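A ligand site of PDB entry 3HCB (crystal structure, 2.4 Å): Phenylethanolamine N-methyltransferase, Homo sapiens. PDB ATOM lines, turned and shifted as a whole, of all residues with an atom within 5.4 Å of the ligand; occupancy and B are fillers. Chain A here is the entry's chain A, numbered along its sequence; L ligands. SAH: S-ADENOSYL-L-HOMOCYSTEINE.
The side-chain hydroxyl of Tyr 35 lies within hydrogen-bond range of an oxygen (OXT) of the ligand (2.5 Å).
The backbone carbonyl oxygen of Ala 181 lies within hydrogen-bond range of a nitrogen (N) of the ligand (2.7 Å).
OXT of the ligand sits at hydrogen-bond distance from OH of Tyr 40, 2.7 Å away.
OH of Tyr 85 is in hydrogen-bond range of O of the ligand.
An oxygen (O3') of the ligand sits at hydrogen-bond distance from the side-chain amide oxygen of Asn 106.
O of Gly 79 lies within hydrogen-bond range of N of the ligand (2.9 Å).
OD2 of Asp 101 lies within hydrogen-bond range of O2' of the ligand, at 3.0 Å.
A nitrogen (N) of the ligand sits close to the backbone carbonyl oxygen (O) of Ser 80 (3.2 Å).
N of Val 159 lies within hydrogen-bond range of N1 of the ligand, at 3.0 Å.
A nitrogen (N6) of the ligand is in hydrogen-bond range of the side-chain carboxylate (OD1) of Asp 158, 3.2 Å away.
SG of Cys 183 is in hydrogen-bond range of N3 of the ligand, 3.5 Å away.
The side-chain hydroxyl (OH) of Tyr 40 sits close to the side-chain hydroxyl (OH) of Tyr 85, at 3.0 Å.
NZ of Lys 57 lies within hydrogen-bond range of OH of Tyr 40 (3.1 Å).
The backbone NH (N) of Leu 103 is in hydrogen-bond range of the side-chain carboxylate (OD2) of Asp 101 (3.2 Å).
The backbone carbonyl oxygen of Ser 80 is in hydrogen-bond range of the side-chain hydroxyl of Thr 83.
The backbone carbonyl oxygen (O) of Ser 80 lies within hydrogen-bond range of the side-chain amide nitrogen (NE2) of Gln 86, at 3.4 Å.
OD1 of Asp 158 lies within hydrogen-bond range of N of His 160 (2.6 Å).
OG1 of Thr 83 sits at hydrogen-bond distance from OE1 of Gln 86 (2.7 Å).
OH of Tyr 27 sits at hydrogen-bond distance from OH of Tyr 222, at 2.9 Å.
O of Phe 182 sits close to SD of the ligand, at 3.5 Å.
Tyr 27 touches the ligand (CE2 to C2', 3.6 Å).
Gly 81 touches the ligand (CA to O3', 3.4 Å).
Thr 83 touches the ligand.
CB of Phe 102 touches C4 of the ligand, 3.3 Å away.
Leu 103 touches the ligand (CG to O2', 3.6 Å).
Ile 157 touches the ligand.
His 160 touches the ligand (ND1 to N6, 3.5 Å).
CG1 of Val 187 touches N7 of the ligand, at 3.4 Å.
Within 4 Å of the ligand: Tyr 27, Tyr 35, Tyr 40, Gly 79, Ser 80, Gly 81, Thr 83, Tyr 85, Asp 101, Phe 102, Leu 103, Asn 106, Ile 157, Asp 158, Val 159, His 160, Ala 181, Phe 182, Cys 183 and Val 187.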
ATOM      1  N   TYR A  27       6.988 -11.344  18.133  1.00  0.00           N
ATOM      2  CA  TYR A  27       5.622 -11.398  17.618  1.00  0.00           C
ATOM      3  C   TYR A  27       4.966 -12.740  17.855  1.00  0.00           C
ATOM      4  O   TYR A  27       3.839 -12.978  17.435  1.00  0.00           O
ATOM      5  CB  TYR A  27       5.586 -11.040  16.128  1.00  0.00           C
ATOM      6  CG  TYR A  27       5.486  -9.562  15.896  1.00  0.00           C
ATOM      7  CD1 TYR A  27       6.600  -8.807  15.574  1.00  0.00           C
ATOM      8  CD2 TYR A  27       4.263  -8.904  16.035  1.00  0.00           C
ATOM      9  CE1 TYR A  27       6.507  -7.449  15.384  1.00  0.00           C
ATOM     10  CE2 TYR A  27       4.168  -7.554  15.839  1.00  0.00           C
ATOM     11  CZ  TYR A  27       5.285  -6.829  15.518  1.00  0.00           C
ATOM     12  OH  TYR A  27       5.173  -5.466  15.331  1.00  0.00           O
ATOM     13  N   PHE A  30       2.515 -12.178  20.725  1.00  0.00           N
ATOM     14  CA  PHE A  30       1.512 -11.189  20.318  1.00  0.00           C
ATOM     15  C   PHE A  30       0.067 -11.679  20.490  1.00  0.00           C
ATOM     16  O   PHE A  30      -0.364 -12.608  19.796  1.00  0.00           O
ATOM     17  CB  PHE A  30       1.782 -10.795  18.864  1.00  0.00           C
ATOM     18  CG  PHE A  30       0.826  -9.774  18.304  1.00  0.00           C
ATOM     19  CD1 PHE A  30       1.207  -8.450  18.206  1.00  0.00           C
ATOM     20  CD2 PHE A  30      -0.431 -10.146  17.856  1.00  0.00           C
ATOM     21  CE1 PHE A  30       0.342  -7.505  17.680  1.00  0.00           C
ATOM     22  CE2 PHE A  30      -1.299  -9.214  17.332  1.00  0.00           C
ATOM     23  CZ  PHE A  30      -0.916  -7.889  17.247  1.00  0.00           C
ATOM     24  N   TYR A  35      -4.171  -6.591  21.870  1.00  0.00           N
ATOM     25  CA  TYR A  35      -3.816  -5.527  20.953  1.00  0.00           C
ATOM     26  C   TYR A  35      -5.054  -4.701  20.567  1.00  0.00           C
ATOM     27  O   TYR A  35      -5.028  -3.476  20.625  1.00  0.00           O
ATOM     28  CB  TYR A  35      -3.112  -6.084  19.721  1.00  0.00           C
ATOM     29  CG  TYR A  35      -2.861  -5.056  18.651  1.00  0.00           C
ATOM     30  CD1 TYR A  35      -1.798  -4.159  18.743  1.00  0.00           C
ATOM     31  CD2 TYR A  35      -3.698  -4.965  17.531  1.00  0.00           C
ATOM     32  CE1 TYR A  35      -1.573  -3.209  17.776  1.00  0.00           C
ATOM     33  CE2 TYR A  35      -3.474  -4.017  16.549  1.00  0.00           C
ATOM     34  CZ  TYR A  35      -2.413  -3.145  16.672  1.00  0.00           C
ATOM     35  OH  TYR A  35      -2.190  -2.203  15.699  1.00  0.00           O
ATOM     36  N   TYR A  40      -8.081  -0.171  20.051  1.00  0.00           N
ATOM     37  CA  TYR A  40      -9.361  -0.023  19.358  1.00  0.00           C
ATOM     38  C   TYR A  40     -10.581  -0.029  20.272  1.00  0.00           C
ATOM     39  O   TYR A  40     -11.713   0.154  19.825  1.00  0.00           O
ATOM     40  CB  TYR A  40      -9.450  -1.025  18.204  1.00  0.00           C
ATOM     41  CG  TYR A  40      -8.371  -0.721  17.177  1.00  0.00           C
ATOM     42  CD1 TYR A  40      -7.130  -1.334  17.233  1.00  0.00           C
ATOM     43  CD2 TYR A  40      -8.579   0.247  16.199  1.00  0.00           C
ATOM     44  CE1 TYR A  40      -6.140  -1.034  16.315  1.00  0.00           C
ATOM     45  CE2 TYR A  40      -7.609   0.551  15.284  1.00  0.00           C
ATOM     46  CZ  TYR A  40      -6.383  -0.087  15.344  1.00  0.00           C
ATOM     47  OH  TYR A  40      -5.401   0.222  14.433  1.00  0.00           O
ATOM     48  N   LYS A  57      -7.912   8.956  11.641  1.00  0.00           N
ATOM     49  CA  LYS A  57      -7.525   7.891  10.723  1.00  0.00           C
ATOM     50  C   LYS A  57      -8.597   7.619   9.664  1.00  0.00           C
ATOM     51  O   LYS A  57      -8.296   7.602   8.469  1.00  0.00           O
ATOM     52  CB  LYS A  57      -7.208   6.600  11.489  1.00  0.00           C
ATOM     53  CG  LYS A  57      -6.015   6.722  12.416  1.00  0.00           C
ATOM     54  CD  LYS A  57      -5.450   5.363  12.788  1.00  0.00           C
ATOM     55  CE  LYS A  57      -6.303   4.658  13.819  1.00  0.00           C
ATOM     56  NZ  LYS A  57      -5.792   3.289  14.049  1.00  0.00           N
ATOM     57  N   ILE A  78      -1.570  -4.792   3.669  1.00  0.00           N
ATOM     58  CA  ILE A  78      -0.304  -5.344   4.154  1.00  0.00           C
ATOM     59  C   ILE A  78      -0.233  -5.357   5.673  1.00  0.00           C
ATOM     60  O   ILE A  78      -0.176  -4.307   6.305  1.00  0.00           O
ATOM     61  CB  ILE A  78       0.897  -4.510   3.655  1.00  0.00           C
ATOM     62  CG1 ILE A  78       0.843  -4.297   2.135  1.00  0.00           C
ATOM     63  CG2 ILE A  78       2.206  -5.152   4.082  1.00  0.00           C
ATOM     64  CD1 ILE A  78       0.861  -5.573   1.319  1.00  0.00           C
ATOM     65  N   GLY A  79      -0.197  -6.544   6.262  1.00  0.00           N
ATOM     66  CA  GLY A  79      -0.078  -6.663   7.708  1.00  0.00           C
ATOM     67  C   GLY A  79      -1.333  -6.173   8.409  1.00  0.00           C
ATOM     68  O   GLY A  79      -1.284  -5.355   9.316  1.00  0.00           O
ATOM     69  N   SER A  80      -2.474  -6.703   7.953  1.00  0.00           N
ATOM     70  CA  SER A  80      -3.790  -6.295   8.439  1.00  0.00           C
ATOM     71  C   SER A  80      -3.911  -6.410   9.952  1.00  0.00           C
ATOM     72  O   SER A  80      -4.679  -5.668  10.579  1.00  0.00           O
ATOM     73  CB  SER A  80      -4.874  -7.163   7.795  1.00  0.00           C
ATOM     74  OG  SER A  80      -4.759  -7.174   6.385  1.00  0.00           O
ATOM     75  N   GLY A  81      -3.170  -7.343  10.533  1.00  0.00           N
ATOM     76  CA  GLY A  81      -3.348  -7.669  11.933  1.00  0.00           C
ATOM     77  C   GLY A  81      -4.747  -8.204  12.136  1.00  0.00           C
ATOM     78  O   GLY A  81      -5.319  -8.822  11.235  1.00  0.00           O
ATOM     79  N   PRO A  82      -5.322  -7.986  13.327  1.00  0.00           N
ATOM     80  CA  PRO A  82      -6.700  -8.412  13.569  1.00  0.00           C
ATOM     81  C   PRO A  82      -7.699  -7.272  13.368  1.00  0.00           C
ATOM     82  O   PRO A  82      -8.717  -7.247  14.047  1.00  0.00           O
ATOM     83  CB  PRO A  82      -6.658  -8.780  15.051  1.00  0.00           C
ATOM     84  CG  PRO A  82      -5.721  -7.753  15.636  1.00  0.00           C
ATOM     85  CD  PRO A  82      -4.714  -7.403  14.539  1.00  0.00           C
ATOM     86  N   THR A  83      -7.401  -6.355  12.455  1.00  0.00           N
ATOM     87  CA  THR A  83      -8.241  -5.163  12.332  1.00  0.00           C
ATOM     88  C   THR A  83      -8.767  -4.985  10.912  1.00  0.00           C
ATOM     89  O   THR A  83      -8.121  -5.391   9.959  1.00  0.00           O
ATOM     90  CB  THR A  83      -7.481  -3.884  12.779  1.00  0.00           C
ATOM     91  OG1 THR A  83      -6.592  -3.451  11.731  1.00  0.00           O
ATOM     92  CG2 THR A  83      -6.681  -4.139  14.059  1.00  0.00           C
ATOM     93  N   TYR A  85     -10.843  -1.827  10.155  1.00  0.00           N
ATOM     94  CA  TYR A  85     -11.249  -0.434   9.963  1.00  0.00           C
ATOM     95  C   TYR A  85     -10.540   0.194   8.781  1.00  0.00           C
ATOM     96  O   TYR A  85     -11.073   1.086   8.126  1.00  0.00           O
ATOM     97  CB  TYR A  85     -10.920   0.391  11.205  1.00  0.00           C
ATOM     98  CG  TYR A  85      -9.451   0.674  11.330  1.00  0.00           C
ATOM     99  CD1 TYR A  85      -8.895   1.826  10.799  1.00  0.00           C
ATOM    100  CD2 TYR A  85      -8.605  -0.235  11.951  1.00  0.00           C
ATOM    101  CE1 TYR A  85      -7.534   2.071  10.886  1.00  0.00           C
ATOM    102  CE2 TYR A  85      -7.255  -0.001  12.055  1.00  0.00           C
ATOM    103  CZ  TYR A  85      -6.720   1.149  11.520  1.00  0.00           C
ATOM    104  OH  TYR A  85      -5.370   1.377  11.632  1.00  0.00           O
ATOM    105  N   GLN A  86      -9.314  -0.251   8.520  1.00  0.00           N
ATOM    106  CA  GLN A  86      -8.466   0.352   7.482  1.00  0.00           C
ATOM    107  C   GLN A  86      -8.966   0.080   6.066  1.00  0.00           C
ATOM    108  O   GLN A  86      -8.439   0.634   5.112  1.00  0.00           O
ATOM    109  CB  GLN A  86      -7.004  -0.097   7.636  1.00  0.00           C
ATOM    110  CG  GLN A  86      -6.711  -1.554   7.297  1.00  0.00           C
ATOM    111  CD  GLN A  86      -6.811  -2.471   8.508  1.00  0.00           C
ATOM    112  OE1 GLN A  86      -7.383  -2.110   9.545  1.00  0.00           O
ATOM    113  NE2 GLN A  86      -6.259  -3.674   8.383  1.00  0.00           N
ATOM    114  N   ASP A 101      -1.417 -11.172   6.894  1.00  0.00           N
ATOM    115  CA  ASP A 101      -0.654 -10.993   8.130  1.00  0.00           C
ATOM    116  C   ASP A 101       0.323 -12.111   8.427  1.00  0.00           C
ATOM    117  O   ASP A 101       0.096 -13.281   8.103  1.00  0.00           O
ATOM    118  CB  ASP A 101      -1.556 -10.759   9.329  1.00  0.00           C
ATOM    119  CG  ASP A 101      -0.835 -10.042  10.450  1.00  0.00           C
ATOM    120  OD1 ASP A 101      -0.443  -8.869  10.252  1.00  0.00           O
ATOM    121  OD2 ASP A 101      -0.630 -10.650  11.520  1.00  0.00           O
ATOM    122  N   PHE A 102       1.421 -11.741   9.072  1.00  0.00           N
ATOM    123  CA  PHE A 102       2.477 -12.665   9.444  1.00  0.00           C
ATOM    124  C   PHE A 102       1.980 -13.743  10.407  1.00  0.00           C
ATOM    125  O   PHE A 102       2.342 -14.911  10.275  1.00  0.00           O
ATOM    126  CB  PHE A 102       3.631 -11.887  10.083  1.00  0.00           C
ATOM    127  CG  PHE A 102       4.838 -12.719  10.410  1.00  0.00           C
ATOM    128  CD1 PHE A 102       5.783 -12.998   9.436  1.00  0.00           C
ATOM    129  CD2 PHE A 102       5.037 -13.179  11.693  1.00  0.00           C
ATOM    130  CE1 PHE A 102       6.898 -13.761   9.738  1.00  0.00           C
ATOM    131  CE2 PHE A 102       6.152 -13.948  12.002  1.00  0.00           C
ATOM    132  CZ  PHE A 102       7.084 -14.232  11.024  1.00  0.00           C
ATOM    133  N   LEU A 103       1.155 -13.347  11.367  1.00  0.00           N
ATOM    134  CA  LEU A 103       0.716 -14.277  12.404  1.00  0.00           C
ATOM    135  C   LEU A 103      -0.524 -15.078  12.003  1.00  0.00           C
ATOM    136  O   LEU A 103      -1.459 -14.547  11.401  1.00  0.00           O
ATOM    137  CB  LEU A 103       0.461 -13.545  13.717  1.00  0.00           C
ATOM    138  CG  LEU A 103       1.704 -12.985  14.399  1.00  0.00           C
ATOM    139  CD1 LEU A 103       1.338 -12.272  15.703  1.00  0.00           C
ATOM    140  CD2 LEU A 103       2.707 -14.105  14.670  1.00  0.00           C
ATOM    141  N   ASN A 106      -3.629 -13.827  14.014  1.00  0.00           N
ATOM    142  CA  ASN A 106      -4.265 -12.647  13.450  1.00  0.00           C
ATOM    143  C   ASN A 106      -5.166 -12.950  12.259  1.00  0.00           C
ATOM    144  O   ASN A 106      -6.193 -12.313  12.066  1.00  0.00           O
ATOM    145  CB  ASN A 106      -3.226 -11.598  13.055  1.00  0.00           C
ATOM    146  CG  ASN A 106      -2.826 -10.738  14.226  1.00  0.00           C
ATOM    147  OD1 ASN A 106      -1.754 -10.130  14.221  1.00  0.00           O
ATOM    148  ND2 ASN A 106      -3.683 -10.678  15.243  1.00  0.00           N
ATOM    149  N   ILE A 157       2.060 -13.430   5.055  1.00  0.00           N
ATOM    150  CA  ILE A 157       2.939 -12.471   4.419  1.00  0.00           C
ATOM    151  C   ILE A 157       4.124 -12.159   5.335  1.00  0.00           C
ATOM    152  O   ILE A 157       4.000 -12.239   6.551  1.00  0.00           O
ATOM    153  CB  ILE A 157       2.186 -11.163   4.059  1.00  0.00           C
ATOM    154  CG1 ILE A 157       3.071 -10.258   3.197  1.00  0.00           C
ATOM    155  CG2 ILE A 157       1.732 -10.449   5.320  1.00  0.00           C
ATOM    156  CD1 ILE A 157       2.396  -8.956   2.810  1.00  0.00           C
ATOM    157  N   ASP A 158       5.257 -11.839   4.729  1.00  0.00           N
ATOM    158  CA  ASP A 158       6.444 -11.364   5.454  1.00  0.00           C
ATOM    159  C   ASP A 158       7.074 -10.251   4.633  1.00  0.00           C
ATOM    160  O   ASP A 158       7.613 -10.507   3.551  1.00  0.00           O
ATOM    161  CB  ASP A 158       7.466 -12.489   5.644  1.00  0.00           C
ATOM    162  CG  ASP A 158       8.679 -12.048   6.460  1.00  0.00           C
ATOM    163  OD1 ASP A 158       8.962 -10.831   6.513  1.00  0.00           O
ATOM    164  OD2 ASP A 158       9.350 -12.922   7.034  1.00  0.00           O
ATOM    165  N   VAL A 159       7.007  -9.026   5.130  1.00  0.00           N
ATOM    166  CA  VAL A 159       7.494  -7.883   4.351  1.00  0.00           C
ATOM    167  C   VAL A 159       9.008  -7.913   4.232  1.00  0.00           C
ATOM    168  O   VAL A 159       9.604  -7.175   3.448  1.00  0.00           O
ATOM    169  CB  VAL A 159       7.009  -6.547   4.930  1.00  0.00           C
ATOM    170  CG1 VAL A 159       5.497  -6.467   4.831  1.00  0.00           C
ATOM    171  CG2 VAL A 159       7.490  -6.370   6.369  1.00  0.00           C
ATOM    172  N   HIS A 160       9.630  -8.775   5.021  1.00  0.00           N
ATOM    173  CA  HIS A 160      11.099  -8.885   5.014  1.00  0.00           C
ATOM    174  C   HIS A 160      11.598  -9.731   3.856  1.00  0.00           C
ATOM    175  O   HIS A 160      12.843  -9.751   3.585  1.00  0.00           O
ATOM    176  CB  HIS A 160      11.576  -9.432   6.359  1.00  0.00           C
ATOM    177  CG  HIS A 160      11.363  -8.458   7.484  1.00  0.00           C
ATOM    178  ND1 HIS A 160      10.848  -8.834   8.719  1.00  0.00           N
ATOM    179  CD2 HIS A 160      11.540  -7.123   7.540  1.00  0.00           C
ATOM    180  CE1 HIS A 160      10.774  -7.760   9.492  1.00  0.00           C
ATOM    181  NE2 HIS A 160      11.168  -6.711   8.800  1.00  0.00           N
ATOM    182  N   ALA A 181      -1.271  -0.252   7.512  1.00  0.00           N
ATOM    183  CA  ALA A 181      -1.358   0.549   8.722  1.00  0.00           C
ATOM    184  C   ALA A 181      -0.588  -0.091   9.875  1.00  0.00           C
ATOM    185  O   ALA A 181      -0.852  -1.232  10.251  1.00  0.00           O
ATOM    186  CB  ALA A 181      -2.812   0.746   9.115  1.00  0.00           C
ATOM    187  N   PHE A 182       0.367   0.650  10.418  1.00  0.00           N
ATOM    188  CA  PHE A 182       1.067   0.237  11.639  1.00  0.00           C
ATOM    189  C   PHE A 182       1.792  -1.108  11.511  1.00  0.00           C
ATOM    190  O   PHE A 182       1.847  -1.882  12.472  1.00  0.00           O
ATOM    191  CB  PHE A 182       0.103   0.228  12.814  1.00  0.00           C
ATOM    192  CG  PHE A 182      -0.518   1.565  13.099  1.00  0.00           C
ATOM    193  CD1 PHE A 182      -1.837   1.829  12.734  1.00  0.00           C
ATOM    194  CD2 PHE A 182       0.209   2.570  13.705  1.00  0.00           C
ATOM    195  CE1 PHE A 182      -2.404   3.070  12.980  1.00  0.00           C
ATOM    196  CE2 PHE A 182      -0.346   3.809  13.964  1.00  0.00           C
ATOM    197  CZ  PHE A 182      -1.659   4.056  13.599  1.00  0.00           C
ATOM    198  N   CYS A 183       2.345  -1.384  10.335  1.00  0.00           N
ATOM    199  CA  CYS A 183       3.046  -2.639  10.111  1.00  0.00           C
ATOM    200  C   CYS A 183       4.566  -2.448  10.019  1.00  0.00           C
ATOM    201  O   CYS A 183       5.298  -2.842  10.932  1.00  0.00           O
ATOM    202  CB  CYS A 183       2.541  -3.311   8.830  1.00  0.00           C
ATOM    203  SG  CYS A 183       3.298  -4.911   8.491  1.00  0.00           S
ATOM    204  N   ALA A 186       6.691  -1.188  12.744  1.00  0.00           N
ATOM    205  CA  ALA A 186       6.509  -2.063  13.894  1.00  0.00           C
ATOM    206  C   ALA A 186       7.124  -3.447  13.714  1.00  0.00           C
ATOM    207  O   ALA A 186       7.137  -4.250  14.648  1.00  0.00           O
ATOM    208  CB  ALA A 186       5.036  -2.179  14.246  1.00  0.00           C
ATOM    209  N   VAL A 187       7.643  -3.724  12.522  1.00  0.00           N
ATOM    210  CA  VAL A 187       8.313  -4.991  12.246  1.00  0.00           C
ATOM    211  C   VAL A 187       9.766  -4.765  11.854  1.00  0.00           C
ATOM    212  O   VAL A 187      10.476  -5.706  11.515  1.00  0.00           O
ATOM    213  CB  VAL A 187       7.619  -5.752  11.102  1.00  0.00           C
ATOM    214  CG1 VAL A 187       6.135  -5.910  11.380  1.00  0.00           C
ATOM    215  CG2 VAL A 187       7.849  -5.044   9.777  1.00  0.00           C
ATOM    216  N   TYR A 222       5.627  -0.998  21.796  1.00  0.00           N
ATOM    217  CA  TYR A 222       4.223  -1.086  22.150  1.00  0.00           C
ATOM    218  C   TYR A 222       3.919  -2.485  22.686  1.00  0.00           C
ATOM    219  O   TYR A 222       4.604  -3.442  22.345  1.00  0.00           O
ATOM    220  CB  TYR A 222       3.308  -0.729  20.974  1.00  0.00           C
ATOM    221  CG  TYR A 222       3.205  -1.805  19.914  1.00  0.00           C
ATOM    222  CD1 TYR A 222       2.172  -2.740  19.948  1.00  0.00           C
ATOM    223  CD2 TYR A 222       4.117  -1.880  18.875  1.00  0.00           C
ATOM    224  CE1 TYR A 222       2.052  -3.717  18.970  1.00  0.00           C
ATOM    225  CE2 TYR A 222       4.019  -2.854  17.900  1.00  0.00           C
ATOM    226  CZ  TYR A 222       2.982  -3.772  17.948  1.00  0.00           C
ATOM    227  OH  TYR A 222       2.868  -4.734  16.982  1.00  0.00           O
HETATM  228  N   SAH L   1      -2.723  -3.115  10.541  1.00  0.00           N
HETATM  229  CA  SAH L   1      -3.331  -3.272  11.847  1.00  0.00           C
HETATM  230  CB  SAH L   1      -2.447  -4.091  12.793  1.00  0.00           C
HETATM  231  CG  SAH L   1      -1.008  -3.578  12.821  1.00  0.00           C
HETATM  232  SD  SAH L   1       0.033  -4.339  14.111  1.00  0.00           S
HETATM  233  C   SAH L   1      -3.648  -1.911  12.469  1.00  0.00           C
HETATM  234  O   SAH L   1      -3.937  -1.032  11.725  1.00  0.00           O
HETATM  235  OXT SAH L   1      -3.818  -1.898  13.852  1.00  0.00           O
HETATM  236  C5' SAH L   1       1.435  -4.894  13.103  1.00  0.00           C
HETATM  237  C4' SAH L   1       1.258  -6.249  12.432  1.00  0.00           C
HETATM  238  O4' SAH L   1       2.410  -6.569  11.737  1.00  0.00           O
HETATM  239  C3' SAH L   1       1.093  -7.392  13.424  1.00  0.00           C
HETATM  240  O3' SAH L   1      -0.194  -7.931  13.265  1.00  0.00           O
HETATM  241  C2' SAH L   1       2.055  -8.292  13.042  1.00  0.00           C
HETATM  242  O2' SAH L   1       1.640  -9.631  13.140  1.00  0.00           O
HETATM  243  C1' SAH L   1       2.371  -7.948  11.705  1.00  0.00           C
HETATM  244  N9  SAH L   1       3.680  -8.472  11.356  1.00  0.00           N
HETATM  245  C8  SAH L   1       4.612  -8.872  12.223  1.00  0.00           C
HETATM  246  N7  SAH L   1       5.718  -9.285  11.513  1.00  0.00           N
HETATM  247  C5  SAH L   1       5.452  -9.120  10.188  1.00  0.00           C
HETATM  248  C6  SAH L   1       6.206  -9.377   9.079  1.00  0.00           C
HETATM  249  N6  SAH L   1       7.544  -9.907   9.236  1.00  0.00           N
HETATM  250  N1  SAH L   1       5.706  -9.126   7.865  1.00  0.00           N
HETATM  251  C2  SAH L   1       4.461  -8.621   7.745  1.00  0.00           C
HETATM  252  N3  SAH L   1       3.714  -8.373   8.847  1.00  0.00           N
HETATM  253  C4  SAH L   1       4.213  -8.625  10.060  1.00  0.00           C
